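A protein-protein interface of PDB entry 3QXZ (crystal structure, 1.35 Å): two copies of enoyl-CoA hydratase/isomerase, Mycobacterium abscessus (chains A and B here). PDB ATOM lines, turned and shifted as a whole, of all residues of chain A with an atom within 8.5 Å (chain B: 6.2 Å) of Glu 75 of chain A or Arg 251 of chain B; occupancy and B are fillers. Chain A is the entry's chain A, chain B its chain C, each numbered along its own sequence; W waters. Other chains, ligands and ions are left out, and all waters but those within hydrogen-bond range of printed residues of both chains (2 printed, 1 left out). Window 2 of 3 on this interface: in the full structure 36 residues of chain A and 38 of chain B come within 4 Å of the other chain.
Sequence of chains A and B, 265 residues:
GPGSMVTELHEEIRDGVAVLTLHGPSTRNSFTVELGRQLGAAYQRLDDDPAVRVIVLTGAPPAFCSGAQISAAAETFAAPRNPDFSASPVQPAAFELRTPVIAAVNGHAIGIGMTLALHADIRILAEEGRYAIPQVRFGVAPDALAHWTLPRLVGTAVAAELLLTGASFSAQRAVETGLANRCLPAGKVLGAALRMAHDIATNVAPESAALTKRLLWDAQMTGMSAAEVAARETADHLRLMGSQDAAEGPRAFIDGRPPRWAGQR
Of chain B, only Arg 251 comes within 4 Å of Glu 75 of chain A.
Arg 251 of chain B touches just one residue of chain A: Glu 75 (2.9 Å).
Of chain A, only Phe 138 (3.7 Å) comes within 4 Å of Gly 249 of chain B.
Pro 250 of chain B touches four residues of chain A.
No residue of chain A comes within 4 Å of Ala 252 of chain B.
Of the printed residues of chain A, Ala 247 of chain B touches Ala 74.
Of the printed residues of chain A, Ile 254 of chain B touches Ser 71.
Printed residues of chain A within 4 Å of Ala 246 of chain B: Phe 138 (3.9 Å).
Of the printed residues of chain B, Ala 74 of chain A touches Ala 247 and Pro 250.
Printed residues of chain B within 4 Å of Ser 71 of chain A: Ile 254 (3.5 Å).
Gly 256 of chain B touches none of the printed residues of chain A.
The nearest residue of chain B that does not touch Glu 75 of chain A is Ala 247 of chain B (5.2 Å).
The nearest residue of chain A that does not touch Arg 251 of chain B is Ala 74 of chain A (4.8 Å).
The nearest printed residue of chain B that does not touch Ala 73 of chain A is Ala 246 of chain B (4.6 Å).
Pro 250 of chain B touches Ile 70 of chain A (CB to O, 3.9 Å).
Ile 70 of chain A touches Phe 253 of chain B.
Ser 71 of chain A touches Ile 254 of chain B.
Pro 250 of chain B touches Ala 73 of chain A (CG to O, 3.9 Å).
Ala 247 of chain B touches Ala 74 of chain A.
Ala 74 of chain A touches Pro 250 of chain B.
Ala 246 of chain B touches Phe 138 of chain A (CA to O, 3.9 Å).
CA of Gly 249 of chain B touches O of Phe 138 of chain A, at 3.7 Å.
Phe 138 of chain A touches Pro 250 of chain B (O to CD, 3.6 Å).
CE1 of Phe 138 of chain A touches CD1 of Phe 253 of chain B (3.7 Å).
The side-chain carboxylate (OE2) of Glu 75 of chain A lies within salt-bridge range of the guanidinium group (NH2) of Arg 251 of chain B (2.9 Å).
Water W2 bridges O of Phe 138 of chain A (2.8 Å) and O of Ala 246 of chain B (2.8 Å).
Water W1 lies within hydrogen-bond range of the backbone carbonyl oxygen of Ala 247 of chain B (2.8 Å), the guanidinium group of Arg 251 of chain B (2.8 Å) and the backbone carbonyl oxygen of Ala 74 of chain A (3.0 Å).
No position is printed for both chains.
Printed residues of chain A that touch a printed residue of chain B: Ile 70, Ser 71, Ala 73, Ala 74, Glu 75 and Phe 138.
Hydrophobic or aromatic side chains of chain B that line the printed part of chain A: Pro 250, Phe 253 and Ile 254.
Among the printed residues, 11 pairs touch across the chains.
Among the printed residues, Asp or Glu carboxylates within 4 Å of a Lys or Arg side-chain nitrogen of the other chain: Glu 75 of chain A with Arg 251 of chain B.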
ATOM      1  N   GLN A  69     -14.006 -31.355  -1.468  1.00  0.00           N
ATOM      2  CA  GLN A  69     -14.023 -29.899  -1.334  1.00  0.00           C
ATOM      3  C   GLN A  69     -14.920 -29.490  -0.152  1.00  0.00           C
ATOM      4  O   GLN A  69     -16.142 -29.535  -0.270  1.00  0.00           O
ATOM      5  CB  GLN A  69     -14.517 -29.285  -2.658  1.00  0.00           C
ATOM      6  CG  GLN A  69     -13.644 -29.704  -3.876  1.00  0.00           C
ATOM      7  CD  GLN A  69     -14.272 -29.453  -5.251  1.00  0.00           C
ATOM      8  OE1 GLN A  69     -15.459 -29.117  -5.376  1.00  0.00           O
ATOM      9  NE2 GLN A  69     -13.464 -29.619  -6.292  1.00  0.00           N
ATOM     10  N   ILE A  70     -14.314 -29.130   0.983  1.00  0.00           N
ATOM     11  CA  ILE A  70     -15.079 -28.862   2.221  1.00  0.00           C
ATOM     12  C   ILE A  70     -15.945 -27.619   2.104  1.00  0.00           C
ATOM     13  O   ILE A  70     -17.138 -27.655   2.445  1.00  0.00           O
ATOM     14  CB  ILE A  70     -14.174 -28.757   3.484  1.00  0.00           C
ATOM     15  CG1 ILE A  70     -13.451 -30.086   3.757  1.00  0.00           C
ATOM     16  CG2 ILE A  70     -14.989 -28.312   4.717  1.00  0.00           C
ATOM     17  CD1 ILE A  70     -14.369 -31.278   3.962  1.00  0.00           C
ATOM     18  N   SER A  71     -15.349 -26.532   1.616  1.00  0.00           N
ATOM     19  CA  SER A  71     -16.068 -25.270   1.440  1.00  0.00           C
ATOM     20  C   SER A  71     -17.297 -25.454   0.550  1.00  0.00           C
ATOM     21  O   SER A  71     -18.294 -24.737   0.695  1.00  0.00           O
ATOM     22  CB  SER A  71     -15.146 -24.185   0.871  1.00  0.00           C
ATOM     23  OG  SER A  71     -14.601 -24.573  -0.382  1.00  0.00           O
ATOM     24  N   ALA A  72     -17.222 -26.438  -0.343  1.00  0.00           N
ATOM     25  CA  ALA A  72     -18.301 -26.751  -1.276  1.00  0.00           C
ATOM     26  C   ALA A  72     -19.253 -27.863  -0.813  1.00  0.00           C
ATOM     27  O   ALA A  72     -20.134 -28.261  -1.573  1.00  0.00           O
ATOM     28  CB  ALA A  72     -17.713 -27.097  -2.649  1.00  0.00           C
ATOM     29  N   ALA A  73     -19.104 -28.340   0.427  1.00  0.00           N
ATOM     30  CA  ALA A  73     -19.874 -29.503   0.917  1.00  0.00           C
ATOM     31  C   ALA A  73     -20.780 -29.240   2.131  1.00  0.00           C
ATOM     32  O   ALA A  73     -21.247 -30.172   2.800  1.00  0.00           O
ATOM     33  CB  ALA A  73     -18.935 -30.680   1.196  1.00  0.00           C
ATOM     34  N   ALA A  74     -21.057 -27.969   2.386  1.00  0.00           N
ATOM     35  CA  ALA A  74     -21.889 -27.571   3.512  1.00  0.00           C
ATOM     36  C   ALA A  74     -23.367 -27.980   3.377  1.00  0.00           C
ATOM     37  O   ALA A  74     -24.042 -28.276   4.374  1.00  0.00           O
ATOM     38  CB  ALA A  74     -21.771 -26.063   3.719  1.00  0.00           C
ATOM     39  N   GLU A  75     -23.864 -27.994   2.144  1.00  0.00           N
ATOM     40  CA  GLU A  75     -25.277 -28.264   1.895  1.00  0.00           C
ATOM     41  C   GLU A  75     -25.441 -29.417   0.930  1.00  0.00           C
ATOM     42  O   GLU A  75     -26.194 -29.335  -0.055  1.00  0.00           O
ATOM     43  CB  GLU A  75     -25.981 -27.020   1.356  1.00  0.00           C
ATOM     44  CG  GLU A  75     -25.857 -25.778   2.253  1.00  0.00           C
ATOM     45  CD  GLU A  75     -26.561 -25.918   3.612  1.00  0.00           C
ATOM     46  OE1 GLU A  75     -27.355 -26.851   3.795  1.00  0.00           O
ATOM     47  OE2 GLU A  75     -26.333 -25.087   4.504  1.00  0.00           O
ATOM     48  N   THR A  76     -24.720 -30.498   1.201  1.00  0.00           N
ATOM     49  CA  THR A  76     -24.873 -31.699   0.395  1.00  0.00           C
ATOM     50  C   THR A  76     -25.842 -32.573   1.145  1.00  0.00           C
ATOM     51  O   THR A  76     -25.460 -33.511   1.854  1.00  0.00           O
ATOM     52  CB  THR A  76     -23.541 -32.414   0.158  1.00  0.00           C
ATOM     53  OG1 THR A  76     -22.575 -31.467  -0.315  1.00  0.00           O
ATOM     54  CG2 THR A  76     -23.708 -33.533  -0.892  1.00  0.00           C
ATOM     55  N   PHE A  77     -27.122 -32.236   1.007  1.00  0.00           N
ATOM     56  CA  PHE A  77     -28.249 -32.923   1.628  1.00  0.00           C
ATOM     57  C   PHE A  77     -28.383 -34.338   1.078  1.00  0.00           C
ATOM     58  O   PHE A  77     -28.025 -34.582  -0.092  1.00  0.00           O
ATOM     59  CB  PHE A  77     -29.570 -32.192   1.293  1.00  0.00           C
ATOM     60  CG  PHE A  77     -29.549 -30.693   1.524  1.00  0.00           C
ATOM     61  CD1 PHE A  77     -29.723 -30.171   2.802  1.00  0.00           C
ATOM     62  CD2 PHE A  77     -29.407 -29.810   0.452  1.00  0.00           C
ATOM     63  CE1 PHE A  77     -29.725 -28.794   3.017  1.00  0.00           C
ATOM     64  CE2 PHE A  77     -29.405 -28.428   0.647  1.00  0.00           C
ATOM     65  CZ  PHE A  77     -29.576 -27.908   1.935  1.00  0.00           C
ATOM     66  N   ALA A  78     -28.976 -35.227   1.855  1.00  0.00           N
ATOM     67  CA  ALA A  78     -29.326 -36.536   1.365  1.00  0.00           C
ATOM     68  C   ALA A  78     -30.657 -36.435   0.580  1.00  0.00           C
ATOM     69  O   ALA A  78     -31.728 -36.821   1.074  1.00  0.00           O
ATOM     70  CB  ALA A  78     -29.427 -37.517   2.529  1.00  0.00           C
ATOM     71  N   ALA A  79     -30.577 -35.890  -0.640  1.00  0.00           N
ATOM     72  CA  ALA A  79     -31.750 -35.727  -1.499  1.00  0.00           C
ATOM     73  C   ALA A  79     -32.174 -37.069  -2.067  1.00  0.00           C
ATOM     74  O   ALA A  79     -31.334 -37.823  -2.553  1.00  0.00           O
ATOM     75  CB  ALA A  79     -31.450 -34.758  -2.632  1.00  0.00           C
ATOM     76  N   PHE A 138     -15.922 -33.769  10.533  1.00  0.00           N
ATOM     77  CA  PHE A 138     -16.807 -32.936   9.733  1.00  0.00           C
ATOM     78  C   PHE A 138     -18.243 -33.407   9.767  1.00  0.00           C
ATOM     79  O   PHE A 138     -19.076 -32.890   9.018  1.00  0.00           O
ATOM     80  CB  PHE A 138     -16.288 -32.866   8.286  1.00  0.00           C
ATOM     81  CG  PHE A 138     -15.004 -32.108   8.163  1.00  0.00           C
ATOM     82  CD1 PHE A 138     -15.013 -30.725   8.026  1.00  0.00           C
ATOM     83  CD2 PHE A 138     -13.780 -32.765   8.217  1.00  0.00           C
ATOM     84  CE1 PHE A 138     -13.825 -30.009   7.937  1.00  0.00           C
ATOM     85  CE2 PHE A 138     -12.572 -32.049   8.125  1.00  0.00           C
ATOM     86  CZ  PHE A 138     -12.601 -30.669   7.985  1.00  0.00           C
ATOM     87  N   ALA B 246     -23.593 -32.768  10.133  1.00  0.00           N
ATOM     88  CA  ALA B 246     -23.000 -32.760   8.796  1.00  0.00           C
ATOM     89  C   ALA B 246     -23.043 -31.370   8.145  1.00  0.00           C
ATOM     90  O   ALA B 246     -22.247 -31.091   7.241  1.00  0.00           O
ATOM     91  CB  ALA B 246     -23.654 -33.789   7.895  1.00  0.00           C
ATOM     92  N   ALA B 247     -23.976 -30.512   8.580  1.00  0.00           N
ATOM     93  CA  ALA B 247     -23.951 -29.106   8.161  1.00  0.00           C
ATOM     94  C   ALA B 247     -22.932 -28.315   8.995  1.00  0.00           C
ATOM     95  O   ALA B 247     -22.171 -27.503   8.454  1.00  0.00           O
ATOM     96  CB  ALA B 247     -25.365 -28.487   8.306  1.00  0.00           C
ATOM     97  N   GLU B 248     -22.896 -28.564  10.300  1.00  0.00           N
ATOM     98  CA  GLU B 248     -22.058 -27.842  11.239  1.00  0.00           C
ATOM     99  C   GLU B 248     -20.565 -28.047  10.998  1.00  0.00           C
ATOM    100  O   GLU B 248     -19.774 -27.115  11.150  1.00  0.00           O
ATOM    101  CB  GLU B 248     -22.445 -28.215  12.679  1.00  0.00           C
ATOM    102  CG  GLU B 248     -21.557 -27.622  13.801  1.00  0.00           C
ATOM    103  CD  GLU B 248     -21.556 -26.083  13.909  1.00  0.00           C
ATOM    104  OE1 GLU B 248     -22.213 -25.369  13.122  1.00  0.00           O
ATOM    105  OE2 GLU B 248     -20.879 -25.608  14.832  1.00  0.00           O
ATOM    106  N   GLY B 249     -20.160 -29.255  10.634  1.00  0.00           N
ATOM    107  CA  GLY B 249     -18.724 -29.504  10.423  1.00  0.00           C
ATOM    108  C   GLY B 249     -18.144 -28.574   9.365  1.00  0.00           C
ATOM    109  O   GLY B 249     -17.198 -27.823   9.653  1.00  0.00           O
ATOM    110  N   PRO B 250     -18.699 -28.589   8.148  1.00  0.00           N
ATOM    111  CA  PRO B 250     -18.236 -27.660   7.095  1.00  0.00           C
ATOM    112  C   PRO B 250     -18.490 -26.191   7.439  1.00  0.00           C
ATOM    113  O   PRO B 250     -17.622 -25.352   7.174  1.00  0.00           O
ATOM    114  CB  PRO B 250     -19.048 -28.070   5.864  1.00  0.00           C
ATOM    115  CG  PRO B 250     -19.390 -29.507   6.110  1.00  0.00           C
ATOM    116  CD  PRO B 250     -19.569 -29.645   7.606  1.00  0.00           C
ATOM    117  N   ARG B 251     -19.643 -25.885   8.031  1.00  0.00           N
ATOM    118  CA  ARG B 251     -19.983 -24.491   8.368  1.00  0.00           C
ATOM    119  C   ARG B 251     -18.969 -23.903   9.343  1.00  0.00           C
ATOM    120  O   ARG B 251     -18.521 -22.751   9.163  1.00  0.00           O
ATOM    121  CB  ARG B 251     -21.404 -24.398   8.939  1.00  0.00           C
ATOM    122  CG  ARG B 251     -22.019 -22.996   8.954  1.00  0.00           C
ATOM    123  CD  ARG B 251     -22.713 -22.668   7.617  1.00  0.00           C
ATOM    124  NE  ARG B 251     -23.842 -23.573   7.324  1.00  0.00           N
ATOM    125  CZ  ARG B 251     -25.114 -23.300   7.614  1.00  0.00           C
ATOM    126  NH1 ARG B 251     -25.423 -22.149   8.204  1.00  0.00           N
ATOM    127  NH2 ARG B 251     -26.076 -24.163   7.288  1.00  0.00           N
ATOM    128  N   ALA B 252     -18.592 -24.680  10.361  1.00  0.00           N
ATOM    129  CA  ALA B 252     -17.599 -24.240  11.345  1.00  0.00           C
ATOM    130  C   ALA B 252     -16.241 -24.043  10.703  1.00  0.00           C
ATOM    131  O   ALA B 252     -15.543 -23.063  11.008  1.00  0.00           O
ATOM    132  CB  ALA B 252     -17.499 -25.193  12.520  1.00  0.00           C
ATOM    133  N   PHE B 253     -15.861 -24.976   9.831  1.00  0.00           N
ATOM    134  CA  PHE B 253     -14.596 -24.917   9.113  1.00  0.00           C
ATOM    135  C   PHE B 253     -14.513 -23.638   8.283  1.00  0.00           C
ATOM    136  O   PHE B 253     -13.522 -22.908   8.369  1.00  0.00           O
ATOM    137  CB  PHE B 253     -14.446 -26.157   8.218  1.00  0.00           C
ATOM    138  CG  PHE B 253     -13.119 -26.245   7.518  1.00  0.00           C
ATOM    139  CD1 PHE B 253     -11.991 -26.747   8.174  1.00  0.00           C
ATOM    140  CD2 PHE B 253     -13.003 -25.833   6.193  1.00  0.00           C
ATOM    141  CE1 PHE B 253     -10.760 -26.829   7.515  1.00  0.00           C
ATOM    142  CE2 PHE B 253     -11.779 -25.913   5.526  1.00  0.00           C
ATOM    143  CZ  PHE B 253     -10.667 -26.412   6.189  1.00  0.00           C
ATOM    144  N   ILE B 254     -15.559 -23.366   7.500  1.00  0.00           N
ATOM    145  CA  ILE B 254     -15.651 -22.168   6.662  1.00  0.00           C
ATOM    146  C   ILE B 254     -15.601 -20.880   7.508  1.00  0.00           C
ATOM    147  O   ILE B 254     -14.967 -19.891   7.101  1.00  0.00           O
ATOM    148  CB  ILE B 254     -16.932 -22.214   5.770  1.00  0.00           C
ATOM    149  CG1 ILE B 254     -16.855 -23.374   4.761  1.00  0.00           C
ATOM    150  CG2 ILE B 254     -17.147 -20.890   5.042  1.00  0.00           C
ATOM    151  CD1 ILE B 254     -18.198 -23.703   4.083  1.00  0.00           C
ATOM    152  N   ASP B 255     -16.248 -20.892   8.675  1.00  0.00           N
ATOM    153  CA  ASP B 255     -16.216 -19.743   9.600  1.00  0.00           C
ATOM    154  C   ASP B 255     -14.908 -19.576  10.353  1.00  0.00           C
ATOM    155  O   ASP B 255     -14.662 -18.509  10.939  1.00  0.00           O
ATOM    156  CB  ASP B 255     -17.307 -19.871  10.659  1.00  0.00           C
ATOM    157  CG  ASP B 255     -18.658 -19.475  10.165  1.00  0.00           C
ATOM    158  OD1 ASP B 255     -18.798 -19.067   8.988  1.00  0.00           O
ATOM    159  OD2 ASP B 255     -19.603 -19.592  10.974  1.00  0.00           O
ATOM    160  N   GLY B 256     -14.088 -20.617  10.378  1.00  0.00           N
ATOM    161  CA  GLY B 256     -12.877 -20.636  11.199  1.00  0.00           C
ATOM    162  C   GLY B 256     -13.162 -20.583  12.691  1.00  0.00           C
ATOM    163  O   GLY B 256     -12.565 -19.786  13.419  1.00  0.00           O
ATOM    164  N   ARG B 257     -14.084 -21.423  13.153  1.00  0.00           N
ATOM    165  CA  ARG B 257     -14.465 -21.472  14.565  1.00  0.00           C
ATOM    166  C   ARG B 257     -14.602 -22.943  14.985  1.00  0.00           C
ATOM    167  O   ARG B 257     -14.711 -23.820  14.117  1.00  0.00           O
ATOM    168  CB  ARG B 257     -15.797 -20.722  14.777  1.00  0.00           C
ATOM    169  CG  ARG B 257     -16.961 -21.340  13.990  1.00  0.00           C
ATOM    170  CD  ARG B 257     -18.288 -20.651  14.246  1.00  0.00           C
ATOM    171  NE  ARG B 257     -19.337 -21.220  13.403  1.00  0.00           N
ATOM    172  CZ  ARG B 257     -19.952 -22.389  13.637  1.00  0.00           C
ATOM    173  NH1 ARG B 257     -19.649 -23.089  14.722  1.00  0.00           N
ATOM    174  NH2 ARG B 257     -20.891 -22.827  12.801  1.00  0.00           N
HETATM  175  O   HOH W   1     -23.271 -26.134   6.282  1.00  0.00           O
HETATM  176  O   HOH W   2     -20.190 -32.840   6.480  1.00  0.00           O
